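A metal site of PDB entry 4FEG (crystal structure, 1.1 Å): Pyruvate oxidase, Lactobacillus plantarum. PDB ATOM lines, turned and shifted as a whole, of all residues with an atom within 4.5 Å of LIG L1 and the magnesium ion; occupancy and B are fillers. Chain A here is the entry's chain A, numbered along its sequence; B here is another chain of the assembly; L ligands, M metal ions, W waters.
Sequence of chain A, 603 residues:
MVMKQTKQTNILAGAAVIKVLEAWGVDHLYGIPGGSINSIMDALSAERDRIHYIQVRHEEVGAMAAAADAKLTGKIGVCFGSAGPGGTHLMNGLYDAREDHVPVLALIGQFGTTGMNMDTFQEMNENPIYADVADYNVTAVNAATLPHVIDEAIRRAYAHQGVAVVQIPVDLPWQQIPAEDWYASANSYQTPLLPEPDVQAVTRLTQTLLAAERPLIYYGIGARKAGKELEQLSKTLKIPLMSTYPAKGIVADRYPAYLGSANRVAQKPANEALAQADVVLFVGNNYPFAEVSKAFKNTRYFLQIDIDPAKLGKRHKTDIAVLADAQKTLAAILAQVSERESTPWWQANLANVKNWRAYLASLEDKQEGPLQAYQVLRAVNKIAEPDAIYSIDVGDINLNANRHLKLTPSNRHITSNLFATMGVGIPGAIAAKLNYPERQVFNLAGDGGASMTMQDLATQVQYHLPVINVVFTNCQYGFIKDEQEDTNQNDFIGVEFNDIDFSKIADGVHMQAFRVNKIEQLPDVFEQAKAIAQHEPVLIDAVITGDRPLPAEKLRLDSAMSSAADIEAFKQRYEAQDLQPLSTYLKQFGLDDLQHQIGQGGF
The backbone NH (N) of Phe 479 lies within hydrogen-bond range of an oxygen (O5) of LIG L1 (2.9 Å). N of Gly 478 is in hydrogen-bond range of O5 of LIG L1 (3.4 Å). The side-chain amide nitrogen (NE2) of Gln 122 of chain B is in hydrogen-bond range of an oxygen (O8) of LIG L1, 3.1 Å away. N of Gly 448 sits at hydrogen-bond distance from O2 of LIG L1 (3.3 Å). N of Met 422 sits at hydrogen-bond distance from N3 of LIG L1, at 3.3 Å. The backbone NH of Asp 396 lies within hydrogen-bond range of an oxygen (O5) of LIG L1 (2.9 Å). N2 of LIG L1 lies within hydrogen-bond range of O of Ala 420, 2.7 Å away. An oxygen (O2) of LIG L1 sits at hydrogen-bond distance from the backbone NH (N) of Gly 449 (2.9 Å). The side-chain carboxylate (OE2) of Glu 59 of chain B sits at hydrogen-bond distance from a nitrogen (N4) of LIG L1 (2.6 Å).
The side-chain carboxylate of Glu 59 of chain B lies within hydrogen-bond range of a ring nitrogen (ND1) of His 89 of chain B (2.8 Å). N of Asp 447 is in hydrogen-bond range of O of Phe 472. ND2 of Asn 92 lies within hydrogen-bond range of O of Pro 85 of chain B. The side-chain amide nitrogen (ND2) of Asn 92 sits close to a ring nitrogen (NE2) of His 89 of chain B (3.4 Å).
Residues that only touch LIG L1: Ser 82 of chain B, Pro 33 of chain B, His 89 of chain B, Tyr 477, Ile 480, Val 394, Pro 85 of chain B, Gly 446, Met 452, Gly 86 of chain B, Ile 32 of chain B and Gly 395. 24 residues have an atom within 4 Å of LIG L1: Val 394, Gly 395, Asp 396, Ala 420, Met 422, Gly 446, Asp 447, Gly 448, Gly 449, Met 452, Asn 474, Gln 476, Tyr 477, Gly 478, Phe 479, Ile 480, Ile 32 of chain B, Pro 33 of chain B, Glu 59 of chain B, Ser 82 of chain B, Pro 85 of chain B, Gly 86 of chain B, His 89 of chain B and Gln 122 of chain B. The nearest printed residue that does not touch LIG L1 is Thr 421 (4.1 Å).
Along chain A the residues within 4 Å of the magnesium ion span positions 447 to 476. The nearest printed residue that does not touch the magnesium ion is Gly 448 (4.1 Å).
The magnesium ion is bound by an oxygen (O1) of LIG L1, the side-chain carboxylate (OD1) of Asp 447, the backbone carbonyl oxygen (O) of Gln 476, water W4, an oxygen (O4) of LIG L1 and the side-chain amide oxygen (OD1) of Asn 474. The magnesium ion has six donor atoms within binding distance.
Water W4 lies within hydrogen-bond range of the backbone carbonyl oxygen (O) of Phe 472 (2.6 Å), an oxygen (O6) of LIG L1 (2.7 Å), the backbone NH (N) of Asp 447 (3.2 Å) and the side-chain amide nitrogen (ND2) of Asn 474 (3.4 Å). Water W1 lies within hydrogen-bond range of O2 of LIG L1 (2.7 Å), O of Val 394 (2.8 Å) and N of Gly 446 (2.8 Å). Water W3 bridges the side-chain hydroxyl of Ser 82 of chain B (2.7 Å) and the side-chain amide oxygen of Gln 122 of chain B (3.0 Å).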
ATOM      1  N   ASN A  92      15.061 -19.607  -2.392  1.00  0.00           N
ATOM      2  CA  ASN A  92      16.051 -19.828  -1.354  1.00  0.00           C
ATOM      3  C   ASN A  92      16.515 -21.292  -1.314  1.00  0.00           C
ATOM      4  O   ASN A  92      17.638 -21.561  -0.964  1.00  0.00           O
ATOM      5  CB  ASN A  92      15.548 -19.373   0.012  1.00  0.00           C
ATOM      6  CG  ASN A  92      15.748 -17.888   0.159  1.00  0.00           C
ATOM      7  OD1 ASN A  92      15.367 -17.127  -0.746  1.00  0.00           O
ATOM      8  ND2 ASN A  92      16.342 -17.430   1.228  1.00  0.00           N
ATOM      9  N   VAL A 394      20.161 -21.866  10.745  1.00  0.00           N
ATOM     10  CA  VAL A 394      21.316 -20.991  10.515  1.00  0.00           C
ATOM     11  C   VAL A 394      21.320 -19.884  11.569  1.00  0.00           C
ATOM     12  O   VAL A 394      20.326 -19.161  11.749  1.00  0.00           O
ATOM     13  CB  VAL A 394      21.235 -20.390   9.088  1.00  0.00           C
ATOM     14  CG1 VAL A 394      22.219 -19.258   8.889  1.00  0.00           C
ATOM     15  CG2 VAL A 394      21.430 -21.475   8.071  1.00  0.00           C
ATOM     16  N   GLY A 395      22.456 -19.741  12.267  1.00  0.00           N
ATOM     17  CA  GLY A 395      22.620 -18.760  13.290  1.00  0.00           C
ATOM     18  C   GLY A 395      23.536 -19.291  14.379  1.00  0.00           C
ATOM     19  O   GLY A 395      24.397 -20.151  14.126  1.00  0.00           O
ATOM     20  N   ASP A 396      23.343 -18.815  15.622  1.00  0.00           N
ATOM     21  CA  ASP A 396      24.122 -19.346  16.703  1.00  0.00           C
ATOM     22  C   ASP A 396      23.997 -20.861  16.827  1.00  0.00           C
ATOM     23  O   ASP A 396      24.938 -21.484  17.322  1.00  0.00           O
ATOM     24  CB  ASP A 396      23.717 -18.709  18.014  1.00  0.00           C
ATOM     25  CG  ASP A 396      24.258 -17.358  18.339  1.00  0.00           C
ATOM     26  OD1 ASP A 396      25.181 -16.899  17.693  1.00  0.00           O
ATOM     27  OD2 ASP A 396      23.722 -16.763  19.353  1.00  0.00           O
ATOM     28  N   ILE A 397      22.909 -21.459  16.371  1.00  0.00           N
ATOM     29  CA  ILE A 397      22.788 -22.910  16.489  1.00  0.00           C
ATOM     30  C   ILE A 397      23.908 -23.612  15.751  1.00  0.00           C
ATOM     31  O   ILE A 397      24.351 -24.696  16.183  1.00  0.00           O
ATOM     32  CB  ILE A 397      21.391 -23.414  16.029  1.00  0.00           C
ATOM     33  CG1 ILE A 397      21.195 -24.882  16.370  1.00  0.00           C
ATOM     34  CG2 ILE A 397      21.145 -23.186  14.551  1.00  0.00           C
ATOM     35  CD1 ILE A 397      21.361 -25.254  17.863  1.00  0.00           C
ATOM     36  N   ALA A 420      23.691 -20.425   3.250  1.00  0.00           N
ATOM     37  CA  ALA A 420      23.304 -20.181   4.623  1.00  0.00           C
ATOM     38  C   ALA A 420      21.954 -19.522   4.724  1.00  0.00           C
ATOM     39  O   ALA A 420      21.750 -18.557   5.462  1.00  0.00           O
ATOM     40  CB  ALA A 420      24.362 -19.423   5.392  1.00  0.00           C
ATOM     41  N   THR A 421      20.958 -20.085   4.011  1.00  0.00           N
ATOM     42  CA  THR A 421      19.586 -19.602   4.178  1.00  0.00           C
ATOM     43  C   THR A 421      18.990 -20.082   5.514  1.00  0.00           C
ATOM     44  O   THR A 421      18.907 -21.261   5.786  1.00  0.00           O
ATOM     45  CB  THR A 421      18.672 -19.937   2.999  1.00  0.00           C
ATOM     46  OG1 THR A 421      17.396 -19.365   3.218  1.00  0.00           O
ATOM     47  CG2 THR A 421      18.538 -21.447   2.732  1.00  0.00           C
ATOM     48  N   MET A 422      18.530 -19.098   6.296  1.00  0.00           N
ATOM     49  CA  MET A 422      17.695 -19.419   7.435  1.00  0.00           C
ATOM     50  C   MET A 422      16.418 -20.118   6.929  1.00  0.00           C
ATOM     51  O   MET A 422      15.995 -19.941   5.773  1.00  0.00           O
ATOM     52  CB  MET A 422      17.313 -18.143   8.164  1.00  0.00           C
ATOM     53  CG  MET A 422      18.463 -17.454   8.900  1.00  0.00           C
ATOM     54  SD  MET A 422      18.048 -15.792   9.380  1.00  0.00           S
ATOM     55  CE  MET A 422      16.725 -16.043  10.561  1.00  0.00           C
ATOM     56  N   GLY A 446      17.163 -21.730  15.624  1.00  0.00           N
ATOM     57  CA  GLY A 446      16.906 -20.518  16.340  1.00  0.00           C
ATOM     58  C   GLY A 446      15.509 -20.012  16.097  1.00  0.00           C
ATOM     59  O   GLY A 446      14.831 -20.417  15.133  1.00  0.00           O
ATOM     60  N   ASP A 447      15.079 -19.076  16.921  1.00  0.00           N
ATOM     61  CA  ASP A 447      13.740 -18.516  16.783  1.00  0.00           C
ATOM     62  C   ASP A 447      13.550 -17.727  15.501  1.00  0.00           C
ATOM     63  O   ASP A 447      12.489 -17.777  14.867  1.00  0.00           O
ATOM     64  CB  ASP A 447      13.349 -17.680  17.995  1.00  0.00           C
ATOM     65  CG  ASP A 447      14.282 -16.621  18.537  1.00  0.00           C
ATOM     66  OD1 ASP A 447      15.413 -16.452  17.981  1.00  0.00           O
ATOM     67  OD2 ASP A 447      13.874 -15.994  19.527  1.00  0.00           O
ATOM     68  N   GLY A 448      14.581 -17.013  15.033  1.00  0.00           N
ATOM     69  CA  GLY A 448      14.474 -16.301  13.793  1.00  0.00           C
ATOM     70  C   GLY A 448      14.247 -17.198  12.599  1.00  0.00           C
ATOM     71  O   GLY A 448      13.368 -16.969  11.746  1.00  0.00           O
ATOM     72  N   GLY A 449      15.064 -18.259  12.511  1.00  0.00           N
ATOM     73  CA  GLY A 449      14.990 -19.202  11.408  1.00  0.00           C
ATOM     74  C   GLY A 449      13.724 -20.066  11.471  1.00  0.00           C
ATOM     75  O   GLY A 449      13.069 -20.264  10.449  1.00  0.00           O
ATOM     76  N   MET A 452      10.743 -18.213  10.129  1.00  0.00           N
ATOM     77  CA  MET A 452      10.639 -18.038   8.686  1.00  0.00           C
ATOM     78  C   MET A 452       9.900 -19.175   8.025  1.00  0.00           C
ATOM     79  O   MET A 452       9.248 -18.909   7.004  1.00  0.00           O
ATOM     80  CB  MET A 452      12.038 -17.863   8.060  1.00  0.00           C
ATOM     81  CG  MET A 452      12.585 -16.467   8.363  1.00  0.00           C
ATOM     82  SD  MET A 452      14.184 -16.274   7.599  1.00  0.00           S
ATOM     83  CE  MET A 452      14.524 -14.572   8.076  1.00  0.00           C
ATOM     84  N   PHE A 472      15.388 -22.489  19.746  1.00  0.00           N
ATOM     85  CA  PHE A 472      16.244 -21.764  20.697  1.00  0.00           C
ATOM     86  C   PHE A 472      15.782 -20.305  20.715  1.00  0.00           C
ATOM     87  O   PHE A 472      16.122 -19.516  19.844  1.00  0.00           O
ATOM     88  CB  PHE A 472      17.731 -21.889  20.302  1.00  0.00           C
ATOM     89  CG  PHE A 472      18.267 -23.292  20.420  1.00  0.00           C
ATOM     90  CD1 PHE A 472      17.892 -24.343  19.625  1.00  0.00           C
ATOM     91  CD2 PHE A 472      19.174 -23.552  21.448  1.00  0.00           C
ATOM     92  CE1 PHE A 472      18.354 -25.604  19.804  1.00  0.00           C
ATOM     93  CE2 PHE A 472      19.711 -24.794  21.616  1.00  0.00           C
ATOM     94  CZ  PHE A 472      19.288 -25.857  20.825  1.00  0.00           C
ATOM     95  N   ASN A 474      15.839 -16.862  21.919  1.00  0.00           N
ATOM     96  CA  ASN A 474      16.560 -15.791  22.589  1.00  0.00           C
ATOM     97  C   ASN A 474      15.904 -14.433  22.332  1.00  0.00           C
ATOM     98  O   ASN A 474      16.414 -13.439  22.864  1.00  0.00           O
ATOM     99  CB  ASN A 474      18.029 -15.749  22.233  1.00  0.00           C
ATOM    100  CG  ASN A 474      18.300 -15.826  20.772  1.00  0.00           C
ATOM    101  OD1 ASN A 474      17.446 -15.593  19.934  1.00  0.00           O
ATOM    102  ND2 ASN A 474      19.578 -16.087  20.426  1.00  0.00           N
ATOM    103  N   GLN A 476      16.167 -12.784  19.707  1.00  0.00           N
ATOM    104  CA  GLN A 476      17.202 -12.069  19.019  1.00  0.00           C
ATOM    105  C   GLN A 476      17.536 -12.753  17.703  1.00  0.00           C
ATOM    106  O   GLN A 476      17.365 -13.986  17.571  1.00  0.00           O
ATOM    107  CB  GLN A 476      18.500 -12.012  19.826  1.00  0.00           C
ATOM    108  CG  GLN A 476      18.393 -11.379  21.155  1.00  0.00           C
ATOM    109  CD  GLN A 476      19.661 -11.547  21.976  1.00  0.00           C
ATOM    110  OE1 GLN A 476      20.448 -12.435  21.734  1.00  0.00           O
ATOM    111  NE2 GLN A 476      19.896 -10.684  22.896  1.00  0.00           N
ATOM    112  N   TYR A 477      18.129 -11.997  16.817  1.00  0.00           N
ATOM    113  CA  TYR A 477      19.012 -12.549  15.765  1.00  0.00           C
ATOM    114  C   TYR A 477      20.406 -12.546  16.392  1.00  0.00           C
ATOM    115  O   TYR A 477      21.188 -11.613  16.172  1.00  0.00           O
ATOM    116  CB  TYR A 477      18.975 -11.726  14.496  1.00  0.00           C
ATOM    117  CG  TYR A 477      17.617 -11.692  13.781  1.00  0.00           C
ATOM    118  CD1 TYR A 477      16.969 -12.859  13.424  1.00  0.00           C
ATOM    119  CD2 TYR A 477      17.019 -10.492  13.474  1.00  0.00           C
ATOM    120  CE1 TYR A 477      15.747 -12.820  12.777  1.00  0.00           C
ATOM    121  CE2 TYR A 477      15.783 -10.479  12.836  1.00  0.00           C
ATOM    122  CZ  TYR A 477      15.146 -11.632  12.477  1.00  0.00           C
ATOM    123  OH  TYR A 477      13.917 -11.579  11.876  1.00  0.00           O
ATOM    124  N   GLY A 478      20.675 -13.494  17.260  1.00  0.00           N
ATOM    125  CA  GLY A 478      21.852 -13.427  18.106  1.00  0.00           C
ATOM    126  C   GLY A 478      23.141 -13.367  17.344  1.00  0.00           C
ATOM    127  O   GLY A 478      24.048 -12.559  17.650  1.00  0.00           O
ATOM    128  N   PHE A 479      23.241 -14.203  16.295  1.00  0.00           N
ATOM    129  CA  PHE A 479      24.457 -14.219  15.498  1.00  0.00           C
ATOM    130  C   PHE A 479      24.776 -12.837  14.960  1.00  0.00           C
ATOM    131  O   PHE A 479      25.934 -12.464  14.806  1.00  0.00           O
ATOM    132  CB  PHE A 479      24.243 -15.244  14.377  1.00  0.00           C
ATOM    133  CG  PHE A 479      25.473 -15.850  13.760  1.00  0.00           C
ATOM    134  CD1 PHE A 479      26.224 -16.804  14.445  1.00  0.00           C
ATOM    135  CD2 PHE A 479      25.876 -15.511  12.469  1.00  0.00           C
ATOM    136  CE1 PHE A 479      27.318 -17.417  13.783  1.00  0.00           C
ATOM    137  CE2 PHE A 479      26.947 -16.103  11.857  1.00  0.00           C
ATOM    138  CZ  PHE A 479      27.673 -17.062  12.527  1.00  0.00           C
ATOM    139  N   ILE A 480      23.718 -12.086  14.581  1.00  0.00           N
ATOM    140  CA  ILE A 480      23.873 -10.758  13.996  1.00  0.00           C
ATOM    141  C   ILE A 480      24.057  -9.673  15.054  1.00  0.00           C
ATOM    142  O   ILE A 480      24.820  -8.727  14.861  1.00  0.00           O
ATOM    143  CB  ILE A 480      22.692 -10.407  13.078  1.00  0.00           C
ATOM    144  CG1 ILE A 480      22.441 -11.512  12.059  1.00  0.00           C
ATOM    145  CG2 ILE A 480      22.902  -9.058  12.400  1.00  0.00           C
ATOM    146  CD1 ILE A 480      23.661 -11.912  11.306  1.00  0.00           C
ATOM    147  N   ILE B  32      15.651  -7.157   7.376  1.00  0.00           N
ATOM    148  CA  ILE B  32      16.251  -7.984   8.427  1.00  0.00           C
ATOM    149  C   ILE B  32      17.759  -7.783   8.329  1.00  0.00           C
ATOM    150  O   ILE B  32      18.295  -7.862   7.209  1.00  0.00           O
ATOM    151  CB  ILE B  32      15.878  -9.477   8.273  1.00  0.00           C
ATOM    152  CG1 ILE B  32      14.389  -9.652   8.563  1.00  0.00           C
ATOM    153  CG2 ILE B  32      16.761 -10.406   9.122  1.00  0.00           C
ATOM    154  CD1 ILE B  32      13.861 -11.059   8.328  1.00  0.00           C
ATOM    155  N   PRO B  33      18.438  -7.493   9.421  1.00  0.00           N
ATOM    156  CA  PRO B  33      19.881  -7.195   9.344  1.00  0.00           C
ATOM    157  C   PRO B  33      20.689  -8.460   9.098  1.00  0.00           C
ATOM    158  O   PRO B  33      20.262  -9.576   9.293  1.00  0.00           O
ATOM    159  CB  PRO B  33      20.199  -6.581  10.701  1.00  0.00           C
ATOM    160  CG  PRO B  33      19.262  -7.325  11.604  1.00  0.00           C
ATOM    161  CD  PRO B  33      17.965  -7.423  10.788  1.00  0.00           C
ATOM    162  N   GLU B  59      11.926 -11.615   4.935  1.00  0.00           N
ATOM    163  CA  GLU B  59      12.154 -10.486   4.018  1.00  0.00           C
ATOM    164  C   GLU B  59      11.094 -10.350   2.944  1.00  0.00           C
ATOM    165  O   GLU B  59      10.909  -9.250   2.418  1.00  0.00           O
ATOM    166  CB  GLU B  59      13.540 -10.573   3.408  1.00  0.00           C
ATOM    167  CG  GLU B  59      14.666 -10.543   4.405  1.00  0.00           C
ATOM    168  CD  GLU B  59      15.115 -11.881   4.935  1.00  0.00           C
ATOM    169  OE1 GLU B  59      14.388 -12.901   4.802  1.00  0.00           O
ATOM    170  OE2 GLU B  59      16.224 -11.910   5.532  1.00  0.00           O
ATOM    171  N   SER B  82      19.725  -8.971   3.358  1.00  0.00           N
ATOM    172  CA  SER B  82      21.121  -9.321   3.482  1.00  0.00           C
ATOM    173  C   SER B  82      21.584 -10.144   2.303  1.00  0.00           C
ATOM    174  O   SER B  82      20.804 -10.724   1.534  1.00  0.00           O
ATOM    175  CB  SER B  82      21.329 -10.070   4.820  1.00  0.00           C
ATOM    176  OG  SER B  82      20.554 -11.265   4.890  1.00  0.00           O
ATOM    177  N   PRO B  85      20.610 -15.120   0.800  1.00  0.00           N
ATOM    178  CA  PRO B  85      19.222 -15.469   1.109  1.00  0.00           C
ATOM    179  C   PRO B  85      18.366 -14.353   1.611  1.00  0.00           C
ATOM    180  O   PRO B  85      17.119 -14.475   1.512  1.00  0.00           O
ATOM    181  CB  PRO B  85      19.379 -16.556   2.199  1.00  0.00           C
ATOM    182  CG  PRO B  85      20.722 -16.265   2.827  1.00  0.00           C
ATOM    183  CD  PRO B  85      21.557 -15.918   1.623  1.00  0.00           C
ATOM    184  N   GLY B  86      18.893 -13.308   2.199  1.00  0.00           N
ATOM    185  CA  GLY B  86      18.038 -12.192   2.584  1.00  0.00           C
ATOM    186  C   GLY B  86      17.401 -11.541   1.354  1.00  0.00           C
ATOM    187  O   GLY B  86      16.192 -11.348   1.278  1.00  0.00           O
ATOM    188  N   HIS B  89      14.911 -13.743  -0.698  1.00  0.00           N
ATOM    189  CA  HIS B  89      13.595 -13.756  -0.059  1.00  0.00           C
ATOM    190  C   HIS B  89      12.706 -12.572  -0.466  1.00  0.00           C
ATOM    191  O   HIS B  89      11.494 -12.632  -0.272  1.00  0.00           O
ATOM    192  CB  HIS B  89      13.721 -13.768   1.457  1.00  0.00           C
ATOM    193  CG  HIS B  89      13.657 -15.110   2.091  1.00  0.00           C
ATOM    194  ND1 HIS B  89      13.845 -15.258   3.448  1.00  0.00           N
ATOM    195  CD2 HIS B  89      13.319 -16.341   1.652  1.00  0.00           C
ATOM    196  CE1 HIS B  89      13.643 -16.531   3.783  1.00  0.00           C
ATOM    197  NE2 HIS B  89      13.316 -17.225   2.696  1.00  0.00           N
ATOM    198  N   PHE B 121      32.201 -16.832   2.297  1.00  0.00           N
ATOM    199  CA  PHE B 121      30.941 -17.267   2.849  1.00  0.00           C
ATOM    200  C   PHE B 121      29.808 -16.410   2.368  1.00  0.00           C
ATOM    201  O   PHE B 121      29.870 -15.187   2.446  1.00  0.00           O
ATOM    202  CB  PHE B 121      31.042 -17.172   4.375  1.00  0.00           C
ATOM    203  CG  PHE B 121      29.781 -17.518   5.076  1.00  0.00           C
ATOM    204  CD1 PHE B 121      29.360 -18.796   5.249  1.00  0.00           C
ATOM    205  CD2 PHE B 121      28.991 -16.523   5.600  1.00  0.00           C
ATOM    206  CE1 PHE B 121      28.180 -19.119   5.907  1.00  0.00           C
ATOM    207  CE2 PHE B 121      27.808 -16.806   6.254  1.00  0.00           C
ATOM    208  CZ  PHE B 121      27.411 -18.129   6.419  1.00  0.00           C
ATOM    209  N   GLN B 122      28.821 -17.108   1.794  1.00  0.00           N
ATOM    210  CA  GLN B 122      27.579 -16.434   1.350  1.00  0.00           C
ATOM    211  C   GLN B 122      27.882 -15.294   0.384  1.00  0.00           C
ATOM    212  O   GLN B 122      27.170 -14.304   0.281  1.00  0.00           O
ATOM    213  CB  GLN B 122      26.787 -16.012   2.578  1.00  0.00           C
ATOM    214  CG  GLN B 122      25.361 -15.649   2.250  1.00  0.00           C
ATOM    215  CD  GLN B 122      24.791 -15.108   3.527  1.00  0.00           C
ATOM    216  OE1 GLN B 122      25.181 -13.988   3.854  1.00  0.00           O
ATOM    217  NE2 GLN B 122      23.943 -15.843   4.224  1.00  0.00           N
HETATM  218  O1  LIG L   1      17.205 -16.312  15.857  1.00  0.00           O
HETATM  219  P1  LIG L   1      18.129 -16.909  14.830  1.00  0.00           P
HETATM  220  O2  LIG L   1      17.531 -17.929  13.925  1.00  0.00           O
HETATM  221  O3  LIG L   1      19.394 -17.561  15.539  1.00  0.00           O
HETATM  222  P2  LIG L   1      20.284 -17.056  16.825  1.00  0.00           P
HETATM  223  O4  LIG L   1      19.490 -15.974  17.507  1.00  0.00           O
HETATM  224  O5  LIG L   1      21.589 -16.590  16.271  1.00  0.00           O
HETATM  225  O6  LIG L   1      20.358 -18.322  17.638  1.00  0.00           O
HETATM  226  O7  LIG L   1      18.745 -15.691  14.027  1.00  0.00           O
HETATM  227  C1  LIG L   1      19.620 -15.939  12.886  1.00  0.00           C
HETATM  228  C2  LIG L   1      20.244 -14.591  12.576  1.00  0.00           C
HETATM  229  C3  LIG L   1      20.952 -14.568  11.224  1.00  0.00           C
HETATM  230  S1  LIG L   1      22.340 -15.604  10.953  1.00  0.00           S
HETATM  231  C4  LIG L   1      22.446 -15.133   9.298  1.00  0.00           C
HETATM  232  C5  LIG L   1      23.823 -15.189   8.656  1.00  0.00           C
HETATM  233  C6  LIG L   1      24.600 -16.425   9.127  1.00  0.00           C
HETATM  234  O8  LIG L   1      23.703 -15.228   7.260  1.00  0.00           O
HETATM  235  N1  LIG L   1      21.564 -14.018   9.091  1.00  0.00           N
HETATM  236  C7  LIG L   1      20.698 -13.805  10.170  1.00  0.00           C
HETATM  237  C8  LIG L   1      19.624 -12.732  10.054  1.00  0.00           C
HETATM  238  C9  LIG L   1      21.352 -13.392   7.735  1.00  0.00           C
HETATM  239  C10 LIG L   1      20.140 -13.982   6.997  1.00  0.00           C
HETATM  240  C11 LIG L   1      20.165 -15.350   6.489  1.00  0.00           C
HETATM  241  N2  LIG L   1      21.230 -16.123   6.574  1.00  0.00           N
HETATM  242  N3  LIG L   1      19.046 -15.868   5.868  1.00  0.00           N
HETATM  243  C12 LIG L   1      17.993 -15.032   5.688  1.00  0.00           C
HETATM  244  C13 LIG L   1      16.769 -15.566   4.991  1.00  0.00           C
HETATM  245  N4  LIG L   1      17.994 -13.767   6.046  1.00  0.00           N
HETATM  246  C14 LIG L   1      19.086 -13.230   6.726  1.00  0.00           C
HETATM  247  P1  LG2 L   2      32.509 -28.097   0.349  1.00  0.00           P
HETATM  248  O1  LG2 L   2      31.276 -28.765  -0.160  1.00  0.00           O
HETATM  249  O2  LG2 L   2      32.618 -26.626   0.205  1.00  0.00           O
HETATM  250  O3  LG2 L   2      33.816 -28.689  -0.339  1.00  0.00           O
HETATM  251  C1  LG2 L   2      33.996 -30.129  -0.480  1.00  0.00           C
HETATM  252  C2  LG2 L   2      35.311 -30.262  -1.212  1.00  0.00           C
HETATM  253  O4  LG2 L   2      35.562 -31.697  -1.335  1.00  0.00           O
HETATM  254  C3  LG2 L   2      35.299 -29.682  -2.686  1.00  0.00           C
HETATM  255  O5  LG2 L   2      36.511 -28.957  -2.929  1.00  0.00           O
HETATM  256  C4  LG2 L   2      35.174 -30.963  -3.496  1.00  0.00           C
HETATM  257  O6  LG2 L   2      35.669 -30.856  -4.833  1.00  0.00           O
HETATM  258  C5  LG2 L   2      35.946 -31.974  -2.694  1.00  0.00           C
HETATM  259  N1  LG2 L   2      35.591 -33.381  -2.959  1.00  0.00           N
HETATM  260  C6  LG2 L   2      34.332 -33.895  -3.083  1.00  0.00           C
HETATM  261  N2  LG2 L   2      34.373 -35.257  -3.193  1.00  0.00           N
HETATM  262  C7  LG2 L   2      35.708 -35.598  -3.090  1.00  0.00           C
HETATM  263  C8  LG2 L   2      36.384 -36.832  -3.111  1.00  0.00           C
HETATM  264  N3  LG2 L   2      35.793 -37.989  -3.314  1.00  0.00           N
HETATM  265  N4  LG2 L   2      37.738 -36.776  -2.918  1.00  0.00           N
HETATM  266  C9  LG2 L   2      38.396 -35.606  -2.790  1.00  0.00           C
HETATM  267  N5  LG2 L   2      37.786 -34.379  -2.757  1.00  0.00           N
HETATM  268  C10 LG2 L   2      36.441 -34.458  -2.902  1.00  0.00           C
HETATM  269  N6  LG2 L   2      32.537 -23.606   8.254  1.00  0.00           N
HETATM  270  C11 LG2 L   2      33.674 -23.551   9.015  1.00  0.00           C
HETATM  271  O7  LG2 L   2      34.504 -24.500   8.972  1.00  0.00           O
HETATM  272  N7  LG2 L   2      33.871 -22.481   9.842  1.00  0.00           N
HETATM  273  C12 LG2 L   2      32.983 -21.466  10.020  1.00  0.00           C
HETATM  274  O8  LG2 L   2      33.240 -20.481  10.793  1.00  0.00           O
HETATM  275  C13 LG2 L   2      31.769 -21.551   9.279  1.00  0.00           C
HETATM  276  N8  LG2 L   2      30.860 -20.504   9.287  1.00  0.00           N
HETATM  277  C14 LG2 L   2      29.554 -20.870   9.005  1.00  0.00           C
HETATM  278  C15 LG2 L   2      28.477 -20.131   9.470  1.00  0.00           C
HETATM  279  C16 LG2 L   2      27.149 -20.483   9.202  1.00  0.00           C
HETATM  280  C17 LG2 L   2      25.998 -19.657   9.762  1.00  0.00           C
HETATM  281  C18 LG2 L   2      26.918 -21.647   8.416  1.00  0.00           C
HETATM  282  C19 LG2 L   2      25.500 -22.077   8.102  1.00  0.00           C
HETATM  283  C20 LG2 L   2      28.012 -22.361   7.955  1.00  0.00           C
HETATM  284  C21 LG2 L   2      29.318 -22.002   8.200  1.00  0.00           C
HETATM  285  N9  LG2 L   2      30.453 -22.725   7.713  1.00  0.00           N
HETATM  286  C22 LG2 L   2      31.627 -22.624   8.400  1.00  0.00           C
HETATM  287  C23 LG2 L   2      30.370 -23.602   6.549  1.00  0.00           C
HETATM  288  C24 LG2 L   2      31.150 -22.963   5.391  1.00  0.00           C
HETATM  289  O9  LG2 L   2      30.363 -21.855   4.837  1.00  0.00           O
HETATM  290  C25 LG2 L   2      31.541 -23.942   4.276  1.00  0.00           C
HETATM  291  O10 LG2 L   2      30.331 -24.575   3.777  1.00  0.00           O
HETATM  292  C26 LG2 L   2      32.417 -25.069   4.806  1.00  0.00           C
HETATM  293  O11 LG2 L   2      33.526 -24.582   5.626  1.00  0.00           O
HETATM  294  C27 LG2 L   2      33.029 -25.814   3.613  1.00  0.00           C
HETATM  295  O12 LG2 L   2      33.101 -27.214   3.983  1.00  0.00           O
HETATM  296  P2  LG2 L   2      33.722 -28.299   3.024  1.00  0.00           P
HETATM  297  O13 LG2 L   2      34.978 -27.839   2.417  1.00  0.00           O
HETATM  298  O14 LG2 L   2      33.719 -29.552   3.843  1.00  0.00           O
HETATM  299  O15 LG2 L   2      32.612 -28.507   1.879  1.00  0.00           O
HETATM  300 MG    MG M   1      17.384 -16.016  17.838  1.00  0.00          MG
HETATM  301  O   HOH W   1      18.552 -20.388  13.530  1.00  0.00           O
HETATM  302  O   HOH W   2      20.370 -20.393  15.822  1.00  0.00           O
HETATM  303  O   HOH W   3      22.416 -13.177   4.575  1.00  0.00           O
HETATM  304  O   HOH W   4      17.732 -18.036  18.356  1.00  0.00           O
HETATM  305  O   HOH W   5      20.780 -19.735  19.971  1.00  0.00           O
HETATM  306  O   HOH W   6      26.617 -13.498   9.448  1.00  0.00           O
